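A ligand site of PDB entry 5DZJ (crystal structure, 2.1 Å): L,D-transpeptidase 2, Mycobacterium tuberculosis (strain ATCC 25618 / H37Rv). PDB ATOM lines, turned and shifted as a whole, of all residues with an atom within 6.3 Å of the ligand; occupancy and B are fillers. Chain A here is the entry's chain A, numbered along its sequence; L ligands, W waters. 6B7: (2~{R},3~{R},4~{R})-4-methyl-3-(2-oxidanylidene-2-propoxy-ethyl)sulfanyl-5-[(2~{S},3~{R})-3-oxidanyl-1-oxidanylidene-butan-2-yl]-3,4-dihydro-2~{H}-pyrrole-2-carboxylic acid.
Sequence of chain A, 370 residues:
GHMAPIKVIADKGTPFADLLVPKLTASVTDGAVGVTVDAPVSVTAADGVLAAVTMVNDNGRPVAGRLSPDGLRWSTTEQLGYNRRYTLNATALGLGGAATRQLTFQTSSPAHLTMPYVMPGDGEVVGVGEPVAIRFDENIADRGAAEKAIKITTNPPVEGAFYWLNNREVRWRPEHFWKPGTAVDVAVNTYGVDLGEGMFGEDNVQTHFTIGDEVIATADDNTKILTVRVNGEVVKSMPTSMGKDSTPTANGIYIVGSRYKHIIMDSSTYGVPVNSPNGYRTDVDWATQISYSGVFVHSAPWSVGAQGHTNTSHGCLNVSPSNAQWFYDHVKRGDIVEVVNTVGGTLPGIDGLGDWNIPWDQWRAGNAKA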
ATOM      1  N   MET A 265       9.269 -11.941 -22.305  1.00  0.00           N
ATOM      2  CA  MET A 265       8.326 -12.581 -23.214  1.00  0.00           C
ATOM      3  C   MET A 265       7.355 -11.559 -23.756  1.00  0.00           C
ATOM      4  O   MET A 265       6.578 -10.992 -23.009  1.00  0.00           O
ATOM      5  CB  MET A 265       7.529 -13.668 -22.502  1.00  0.00           C
ATOM      6  CG  MET A 265       8.356 -14.686 -21.816  1.00  0.00           C
ATOM      7  SD  MET A 265       9.155 -15.748 -23.010  1.00  0.00           S
ATOM      8  CE  MET A 265       9.389 -17.169 -21.944  1.00  0.00           C
ATOM      9  N   ASP A 266       7.382 -11.355 -25.062  1.00  0.00           N
ATOM     10  CA  ASP A 266       6.557 -10.338 -25.693  1.00  0.00           C
ATOM     11  C   ASP A 266       5.633 -11.035 -26.672  1.00  0.00           C
ATOM     12  O   ASP A 266       6.100 -11.606 -27.666  1.00  0.00           O
ATOM     13  CB  ASP A 266       7.459  -9.310 -26.390  1.00  0.00           C
ATOM     14  CG  ASP A 266       6.701  -8.111 -26.935  1.00  0.00           C
ATOM     15  OD1 ASP A 266       5.457  -8.142 -27.042  1.00  0.00           O
ATOM     16  OD2 ASP A 266       7.380  -7.124 -27.278  1.00  0.00           O
ATOM     17  N   TYR A 270       5.218 -13.090 -31.321  1.00  0.00           N
ATOM     18  CA  TYR A 270       4.541 -14.236 -31.903  1.00  0.00           C
ATOM     19  C   TYR A 270       3.185 -13.869 -32.477  1.00  0.00           C
ATOM     20  O   TYR A 270       2.312 -14.736 -32.583  1.00  0.00           O
ATOM     21  CB  TYR A 270       4.389 -15.343 -30.848  1.00  0.00           C
ATOM     22  CG  TYR A 270       5.669 -15.572 -30.098  1.00  0.00           C
ATOM     23  CD1 TYR A 270       6.784 -16.105 -30.735  1.00  0.00           C
ATOM     24  CD2 TYR A 270       5.783 -15.258 -28.749  1.00  0.00           C
ATOM     25  CE1 TYR A 270       7.977 -16.303 -30.065  1.00  0.00           C
ATOM     26  CE2 TYR A 270       6.970 -15.459 -28.060  1.00  0.00           C
ATOM     27  CZ  TYR A 270       8.064 -15.985 -28.726  1.00  0.00           C
ATOM     28  OH  TYR A 270       9.260 -16.190 -28.067  1.00  0.00           O
ATOM     29  N   ASN A 278      -5.285 -12.410 -25.279  1.00  0.00           N
ATOM     30  CA  ASN A 278      -4.214 -13.393 -25.105  1.00  0.00           C
ATOM     31  C   ASN A 278      -2.829 -12.761 -25.176  1.00  0.00           C
ATOM     32  O   ASN A 278      -1.822 -13.460 -25.247  1.00  0.00           O
ATOM     33  CB  ASN A 278      -4.335 -14.505 -26.149  1.00  0.00           C
ATOM     34  CG  ASN A 278      -5.411 -15.508 -25.804  1.00  0.00           C
ATOM     35  OD1 ASN A 278      -5.609 -15.859 -24.637  1.00  0.00           O
ATOM     36  ND2 ASN A 278      -6.122 -15.966 -26.828  1.00  0.00           N
ATOM     37  N   GLY A 279      -2.794 -11.427 -25.138  1.00  0.00           N
ATOM     38  CA  GLY A 279      -1.541 -10.699 -25.162  1.00  0.00           C
ATOM     39  C   GLY A 279      -0.817 -10.792 -23.838  1.00  0.00           C
ATOM     40  O   GLY A 279      -1.401 -11.117 -22.807  1.00  0.00           O
ATOM     41  N   TYR A 280       0.481 -10.487 -23.858  1.00  0.00           N
ATOM     42  CA  TYR A 280       1.309 -10.525 -22.658  1.00  0.00           C
ATOM     43  C   TYR A 280       2.653  -9.880 -22.916  1.00  0.00           C
ATOM     44  O   TYR A 280       3.153  -9.875 -24.056  1.00  0.00           O
ATOM     45  CB  TYR A 280       1.498 -11.955 -22.177  1.00  0.00           C
ATOM     46  CG  TYR A 280       2.015 -12.889 -23.251  1.00  0.00           C
ATOM     47  CD1 TYR A 280       3.381 -12.968 -23.536  1.00  0.00           C
ATOM     48  CD2 TYR A 280       1.140 -13.671 -24.003  1.00  0.00           C
ATOM     49  CE1 TYR A 280       3.856 -13.809 -24.519  1.00  0.00           C
ATOM     50  CE2 TYR A 280       1.606 -14.520 -24.991  1.00  0.00           C
ATOM     51  CZ  TYR A 280       2.962 -14.585 -25.244  1.00  0.00           C
ATOM     52  OH  TYR A 280       3.441 -15.424 -26.236  1.00  0.00           O
ATOM     53  N   ARG A 281       3.247  -9.342 -21.864  1.00  0.00           N
ATOM     54  CA  ARG A 281       4.630  -8.893 -21.898  1.00  0.00           C
ATOM     55  C   ARG A 281       5.187  -9.046 -20.508  1.00  0.00           C
ATOM     56  O   ARG A 281       4.938  -8.221 -19.629  1.00  0.00           O
ATOM     57  CB  ARG A 281       4.751  -7.463 -22.385  1.00  0.00           C
ATOM     58  CG  ARG A 281       6.188  -7.000 -22.538  1.00  0.00           C
ATOM     59  CD  ARG A 281       6.207  -5.619 -23.149  1.00  0.00           C
ATOM     60  NE  ARG A 281       5.178  -4.828 -22.490  1.00  0.00           N
ATOM     61  CZ  ARG A 281       4.348  -4.009 -23.110  1.00  0.00           C
ATOM     62  NH1 ARG A 281       4.408  -3.843 -24.433  1.00  0.00           N
ATOM     63  NH2 ARG A 281       3.452  -3.359 -22.389  1.00  0.00           N
ATOM     64  N   THR A 282       5.910 -10.149 -20.292  1.00  0.00           N
ATOM     65  CA  THR A 282       6.345 -10.520 -18.960  1.00  0.00           C
ATOM     66  C   THR A 282       7.802 -10.937 -18.946  1.00  0.00           C
ATOM     67  O   THR A 282       8.283 -11.609 -19.858  1.00  0.00           O
ATOM     68  CB  THR A 282       5.484 -11.664 -18.392  1.00  0.00           C
ATOM     69  OG1 THR A 282       5.612 -12.809 -19.242  1.00  0.00           O
ATOM     70  CG2 THR A 282       4.035 -11.262 -18.341  1.00  0.00           C
ATOM     71  N   VAL A 284      10.699 -13.169 -17.419  1.00  0.00           N
ATOM     72  CA  VAL A 284      10.774 -14.465 -16.744  1.00  0.00           C
ATOM     73  C   VAL A 284      12.198 -14.968 -16.663  1.00  0.00           C
ATOM     74  O   VAL A 284      13.043 -14.608 -17.481  1.00  0.00           O
ATOM     75  CB  VAL A 284       9.915 -15.534 -17.453  1.00  0.00           C
ATOM     76  CG1 VAL A 284       8.477 -15.073 -17.571  1.00  0.00           C
ATOM     77  CG2 VAL A 284      10.500 -15.848 -18.827  1.00  0.00           C
ATOM     78  N   SER A 293       6.925 -20.761 -32.125  1.00  0.00           N
ATOM     79  CA  SER A 293       5.629 -20.204 -31.789  1.00  0.00           C
ATOM     80  C   SER A 293       5.599 -19.669 -30.348  1.00  0.00           C
ATOM     81  O   SER A 293       4.594 -19.146 -29.911  1.00  0.00           O
ATOM     82  CB  SER A 293       4.547 -21.254 -32.000  1.00  0.00           C
ATOM     83  OG  SER A 293       4.732 -22.337 -31.109  1.00  0.00           O
ATOM     84  N   GLY A 294       6.705 -19.804 -29.621  1.00  0.00           N
ATOM     85  CA  GLY A 294       6.832 -19.196 -28.302  1.00  0.00           C
ATOM     86  C   GLY A 294       6.674 -20.101 -27.097  1.00  0.00           C
ATOM     87  O   GLY A 294       6.514 -19.612 -25.975  1.00  0.00           O
ATOM     88  N   VAL A 295       6.714 -21.414 -27.287  1.00  0.00           N
ATOM     89  CA  VAL A 295       6.694 -22.302 -26.136  1.00  0.00           C
ATOM     90  C   VAL A 295       8.093 -22.360 -25.523  1.00  0.00           C
ATOM     91  O   VAL A 295       9.100 -22.556 -26.226  1.00  0.00           O
ATOM     92  CB  VAL A 295       6.199 -23.709 -26.501  1.00  0.00           C
ATOM     93  CG1 VAL A 295       6.306 -24.623 -25.298  1.00  0.00           C
ATOM     94  CG2 VAL A 295       4.756 -23.636 -26.985  1.00  0.00           C
ATOM     95  N   PHE A 296       8.131 -22.140 -24.201  1.00  0.00           N
ATOM     96  CA  PHE A 296       9.344 -22.197 -23.385  1.00  0.00           C
ATOM     97  C   PHE A 296       9.113 -23.098 -22.184  1.00  0.00           C
ATOM     98  O   PHE A 296       7.989 -23.234 -21.715  1.00  0.00           O
ATOM     99  CB  PHE A 296       9.737 -20.813 -22.856  1.00  0.00           C
ATOM    100  CG  PHE A 296      10.269 -19.858 -23.891  1.00  0.00           C
ATOM    101  CD1 PHE A 296       9.415 -19.163 -24.731  1.00  0.00           C
ATOM    102  CD2 PHE A 296      11.630 -19.578 -23.948  1.00  0.00           C
ATOM    103  CE1 PHE A 296       9.924 -18.243 -25.652  1.00  0.00           C
ATOM    104  CE2 PHE A 296      12.138 -18.669 -24.871  1.00  0.00           C
ATOM    105  CZ  PHE A 296      11.283 -18.002 -25.718  1.00  0.00           C
ATOM    106  N   HIS A 298      10.196 -22.548 -18.470  1.00  0.00           N
ATOM    107  CA  HIS A 298      10.733 -21.429 -17.706  1.00  0.00           C
ATOM    108  C   HIS A 298      10.257 -21.422 -16.260  1.00  0.00           C
ATOM    109  O   HIS A 298       9.365 -22.175 -15.870  1.00  0.00           O
ATOM    110  CB  HIS A 298      10.349 -20.103 -18.369  1.00  0.00           C
ATOM    111  CG  HIS A 298       8.889 -19.768 -18.249  1.00  0.00           C
ATOM    112  ND1 HIS A 298       8.353 -19.195 -17.117  1.00  0.00           N
ATOM    113  CD2 HIS A 298       7.854 -19.955 -19.106  1.00  0.00           C
ATOM    114  CE1 HIS A 298       7.055 -19.027 -17.278  1.00  0.00           C
ATOM    115  NE2 HIS A 298       6.727 -19.479 -18.485  1.00  0.00           N
ATOM    116  N   ALA A 300       8.385 -20.327 -13.053  1.00  0.00           N
ATOM    117  CA  ALA A 300       7.088 -19.758 -12.769  1.00  0.00           C
ATOM    118  C   ALA A 300       6.789 -19.811 -11.271  1.00  0.00           C
ATOM    119  O   ALA A 300       6.096 -20.695 -10.792  1.00  0.00           O
ATOM    120  CB  ALA A 300       6.012 -20.496 -13.541  1.00  0.00           C
ATOM    121  N   TRP A 302       4.895 -17.934  -9.557  1.00  0.00           N
ATOM    122  CA  TRP A 302       3.472 -17.712  -9.306  1.00  0.00           C
ATOM    123  C   TRP A 302       2.614 -18.969  -9.370  1.00  0.00           C
ATOM    124  O   TRP A 302       1.513 -18.978  -8.833  1.00  0.00           O
ATOM    125  CB  TRP A 302       2.904 -16.680 -10.274  1.00  0.00           C
ATOM    126  CG  TRP A 302       3.036 -17.039 -11.737  1.00  0.00           C
ATOM    127  CD1 TRP A 302       2.134 -17.725 -12.500  1.00  0.00           C
ATOM    128  CD2 TRP A 302       4.133 -16.722 -12.591  1.00  0.00           C
ATOM    129  NE1 TRP A 302       2.606 -17.849 -13.787  1.00  0.00           N
ATOM    130  CE2 TRP A 302       3.835 -17.239 -13.877  1.00  0.00           C
ATOM    131  CE3 TRP A 302       5.348 -16.051 -12.401  1.00  0.00           C
ATOM    132  CZ2 TRP A 302       4.709 -17.119 -14.953  1.00  0.00           C
ATOM    133  CZ3 TRP A 302       6.213 -15.921 -13.478  1.00  0.00           C
ATOM    134  CH2 TRP A 302       5.886 -16.441 -14.743  1.00  0.00           C
ATOM    135  N   SER A 303       3.097 -20.030 -10.017  1.00  0.00           N
ATOM    136  CA  SER A 303       2.232 -21.194 -10.216  1.00  0.00           C
ATOM    137  C   SER A 303       2.760 -22.495  -9.592  1.00  0.00           C
ATOM    138  O   SER A 303       2.290 -23.583  -9.923  1.00  0.00           O
ATOM    139  CB  SER A 303       1.997 -21.420 -11.710  1.00  0.00           C
ATOM    140  OG  SER A 303       3.218 -21.638 -12.393  1.00  0.00           O
ATOM    141  N   THR A 312      -2.266 -24.069 -16.134  1.00  0.00           N
ATOM    142  CA  THR A 312      -2.638 -22.676 -15.974  1.00  0.00           C
ATOM    143  C   THR A 312      -1.949 -21.702 -16.935  1.00  0.00           C
ATOM    144  O   THR A 312      -2.230 -20.501 -16.891  1.00  0.00           O
ATOM    145  CB  THR A 312      -2.335 -22.195 -14.530  1.00  0.00           C
ATOM    146  OG1 THR A 312      -0.918 -22.139 -14.332  1.00  0.00           O
ATOM    147  CG2 THR A 312      -2.972 -23.108 -13.482  1.00  0.00           C
ATOM    148  N   SER A 313      -1.050 -22.177 -17.792  1.00  0.00           N
ATOM    149  CA  SER A 313      -0.258 -21.271 -18.611  1.00  0.00           C
ATOM    150  C   SER A 313      -0.893 -20.930 -19.957  1.00  0.00           C
ATOM    151  O   SER A 313      -1.945 -21.473 -20.331  1.00  0.00           O
ATOM    152  CB  SER A 313       1.143 -21.852 -18.859  1.00  0.00           C
ATOM    153  OG  SER A 313       1.127 -22.814 -19.908  1.00  0.00           O
ATOM    154  N   HIS A 314      -0.230 -20.021 -20.681  1.00  0.00           N
ATOM    155  CA  HIS A 314      -0.555 -19.712 -22.073  1.00  0.00           C
ATOM    156  C   HIS A 314      -0.065 -20.799 -23.059  1.00  0.00           C
ATOM    157  O   HIS A 314      -0.292 -20.722 -24.257  1.00  0.00           O
ATOM    158  CB  HIS A 314       0.052 -18.358 -22.483  1.00  0.00           C
ATOM    159  CG  HIS A 314      -0.656 -17.168 -21.913  1.00  0.00           C
ATOM    160  ND1 HIS A 314      -0.452 -16.721 -20.623  1.00  0.00           N
ATOM    161  CD2 HIS A 314      -1.532 -16.299 -22.475  1.00  0.00           C
ATOM    162  CE1 HIS A 314      -1.190 -15.645 -20.404  1.00  0.00           C
ATOM    163  NE2 HIS A 314      -1.851 -15.367 -21.513  1.00  0.00           N
ATOM    164  N   GLY A 315       0.642 -21.804 -22.546  1.00  0.00           N
ATOM    165  CA  GLY A 315       1.172 -22.853 -23.390  1.00  0.00           C
ATOM    166  C   GLY A 315       2.556 -23.283 -22.949  1.00  0.00           C
ATOM    167  O   GLY A 315       2.999 -24.398 -23.220  1.00  0.00           O
ATOM    168  N   CYS A 316       3.256 -22.386 -22.270  1.00  0.00           N
ATOM    169  CA  CYS A 316       4.587 -22.697 -21.758  1.00  0.00           C
ATOM    170  C   CYS A 316       4.570 -23.854 -20.773  1.00  0.00           C
ATOM    171  O   CYS A 316       3.528 -24.200 -20.209  1.00  0.00           O
ATOM    172  CB  CYS A 316       5.215 -21.474 -21.101  1.00  0.00           C
ATOM    173  SG  CYS A 316       5.702 -20.190 -22.267  1.00  0.00           S
ATOM    174  N   LEU A 317       5.736 -24.463 -20.592  1.00  0.00           N
ATOM    175  CA  LEU A 317       5.892 -25.482 -19.567  1.00  0.00           C
ATOM    176  C   LEU A 317       6.431 -24.762 -18.355  1.00  0.00           C
ATOM    177  O   LEU A 317       7.620 -24.497 -18.229  1.00  0.00           O
ATOM    178  CB  LEU A 317       6.802 -26.622 -20.029  1.00  0.00           C
ATOM    179  CG  LEU A 317       6.170 -27.712 -20.909  1.00  0.00           C
ATOM    180  CD1 LEU A 317       5.493 -27.128 -22.143  1.00  0.00           C
ATOM    181  CD2 LEU A 317       7.194 -28.772 -21.334  1.00  0.00           C
ATOM    182  N   ASN A 318       5.501 -24.394 -17.478  1.00  0.00           N
ATOM    183  CA  ASN A 318       5.831 -23.734 -16.237  1.00  0.00           C
ATOM    184  C   ASN A 318       6.380 -24.752 -15.240  1.00  0.00           C
ATOM    185  O   ASN A 318       5.758 -25.785 -15.017  1.00  0.00           O
ATOM    186  CB  ASN A 318       4.587 -23.057 -15.671  1.00  0.00           C
ATOM    187  CG  ASN A 318       4.276 -21.738 -16.362  1.00  0.00           C
ATOM    188  OD1 ASN A 318       3.855 -20.782 -15.715  1.00  0.00           O
ATOM    189  ND2 ASN A 318       4.499 -21.675 -17.669  1.00  0.00           N
HETATM  190  C10 6B7 L   1       2.486 -15.775 -21.792  1.00  0.00           C
HETATM  191  CD  6B7 L   1       4.676 -16.928 -21.372  1.00  0.00           C
HETATM  192  C12 6B7 L   1       4.178 -17.745 -22.611  1.00  0.00           C
HETATM  193  N   6B7 L   1       4.718 -17.727 -20.124  1.00  0.00           N
HETATM  194  C13 6B7 L   1       4.118 -19.236 -22.321  1.00  0.00           C
HETATM  195  C14 6B7 L   1       4.658 -17.415 -24.048  1.00  0.00           C
HETATM  196  C15 6B7 L   1       6.129 -17.079 -24.281  1.00  0.00           C
HETATM  197  S1  6B7 L   1       1.992 -14.971 -18.976  1.00  0.00           S
HETATM  198  O1  6B7 L   1       0.421 -12.909 -17.766  1.00  0.00           O
HETATM  199  O2  6B7 L   1       1.659 -12.538 -15.860  1.00  0.00           O
HETATM  200  C2  6B7 L   1       2.918 -12.851 -15.234  1.00  0.00           C
HETATM  201  O   6B7 L   1       2.840 -17.973 -17.381  1.00  0.00           O
HETATM  202  C3  6B7 L   1       2.684 -13.735 -14.020  1.00  0.00           C
HETATM  203  OXT 6B7 L   1       2.118 -18.826 -19.374  1.00  0.00           O
HETATM  204  C4  6B7 L   1       1.259 -14.259 -13.919  1.00  0.00           C
HETATM  205  O5  6B7 L   1       3.127 -19.759 -21.843  1.00  0.00           O
HETATM  206  O6  6B7 L   1       4.327 -18.591 -24.781  1.00  0.00           O
HETATM  207  CB  6B7 L   1       3.573 -15.713 -19.584  1.00  0.00           C
HETATM  208  CA  6B7 L   1       3.797 -17.186 -19.370  1.00  0.00           C
HETATM  209  C   6B7 L   1       2.833 -18.087 -18.636  1.00  0.00           C
HETATM  210  CG  6B7 L   1       3.833 -15.682 -21.068  1.00  0.00           C
HETATM  211  O   HOH W   1       1.016 -19.236 -15.323  1.00  0.00           O
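OXT of the ligand is in hydrogen-bond range of N of His 314.
The side-chain sulfur of Cys 316 is covalently linked to a carbon (C13) of the ligand, 1.8 Å away.
The backbone NH (N) of Cys 316 is in hydrogen-bond range of an oxygen (O5) of the ligand, at 2.7 Å.
An oxygen (O6) of the ligand lies within hydrogen-bond range of the backbone carbonyl oxygen of Gly 294 (2.7 Å).
The backbone NH (N) of Gly 315 is in hydrogen-bond range of an oxygen (O5) of the ligand.
A sulfur (S1) of the ligand lies close to a ring nitrogen (ND1) of His 314, at 3.4 Å.
An oxygen (O) of the ligand lies close to the side-chain amide oxygen (OD1) of Asn 318 (3.4 Å).
N of the ligand lies within hydrogen-bond range of NE2 of His 298 (3.1 Å).
ND2 of Asn 318 sits at hydrogen-bond distance from NE2 of His 298, 3.2 Å away.
The side-chain hydroxyl (OG) of Ser 313 lies within hydrogen-bond range of the backbone NH (N) of Gly 315, at 2.9 Å.
O of Thr 282 is in hydrogen-bond range of N of Met 265, 2.7 Å away.
The side-chain hydroxyl (OG) of Ser 303 lies within hydrogen-bond range of the side-chain amide oxygen (OD1) of Asn 318 (3.5 Å).
OG of Ser 313 is in hydrogen-bond range of O of Cys 316 (2.8 Å).
The backbone NH (N) of His 298 lies within hydrogen-bond range of the backbone carbonyl oxygen (O) of Leu 317 (3.2 Å).
The backbone NH (N) of Leu 317 lies within hydrogen-bond range of the backbone carbonyl oxygen (O) of Phe 296 (2.8 Å).
The backbone NH of Phe 296 sits at hydrogen-bond distance from the side-chain sulfur of Cys 316 (3.7 Å).
SD of Met 265 touches C15 of the ligand, 3.5 Å away.
OH of Tyr 280 touches C14 of the ligand (3.2 Å).
Thr 282 touches the ligand (OG1 to CB, 3.6 Å).
Phe 296 touches the ligand (CD1 to C15, 3.9 Å).
Trp 302 touches the ligand.
Ser 313 touches the ligand (CB to OXT, 3.2 Å).
Hydrophobic or aromatic side chains that line the ligand: Met 265, Tyr 280, Phe 296, His 298, Trp 302 and His 314.
Water W1 lies within hydrogen-bond range of NE1 of Trp 302 (2.6 Å), O of the ligand (3.0 Å) and OD1 of Asn 318 (3.3 Å).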
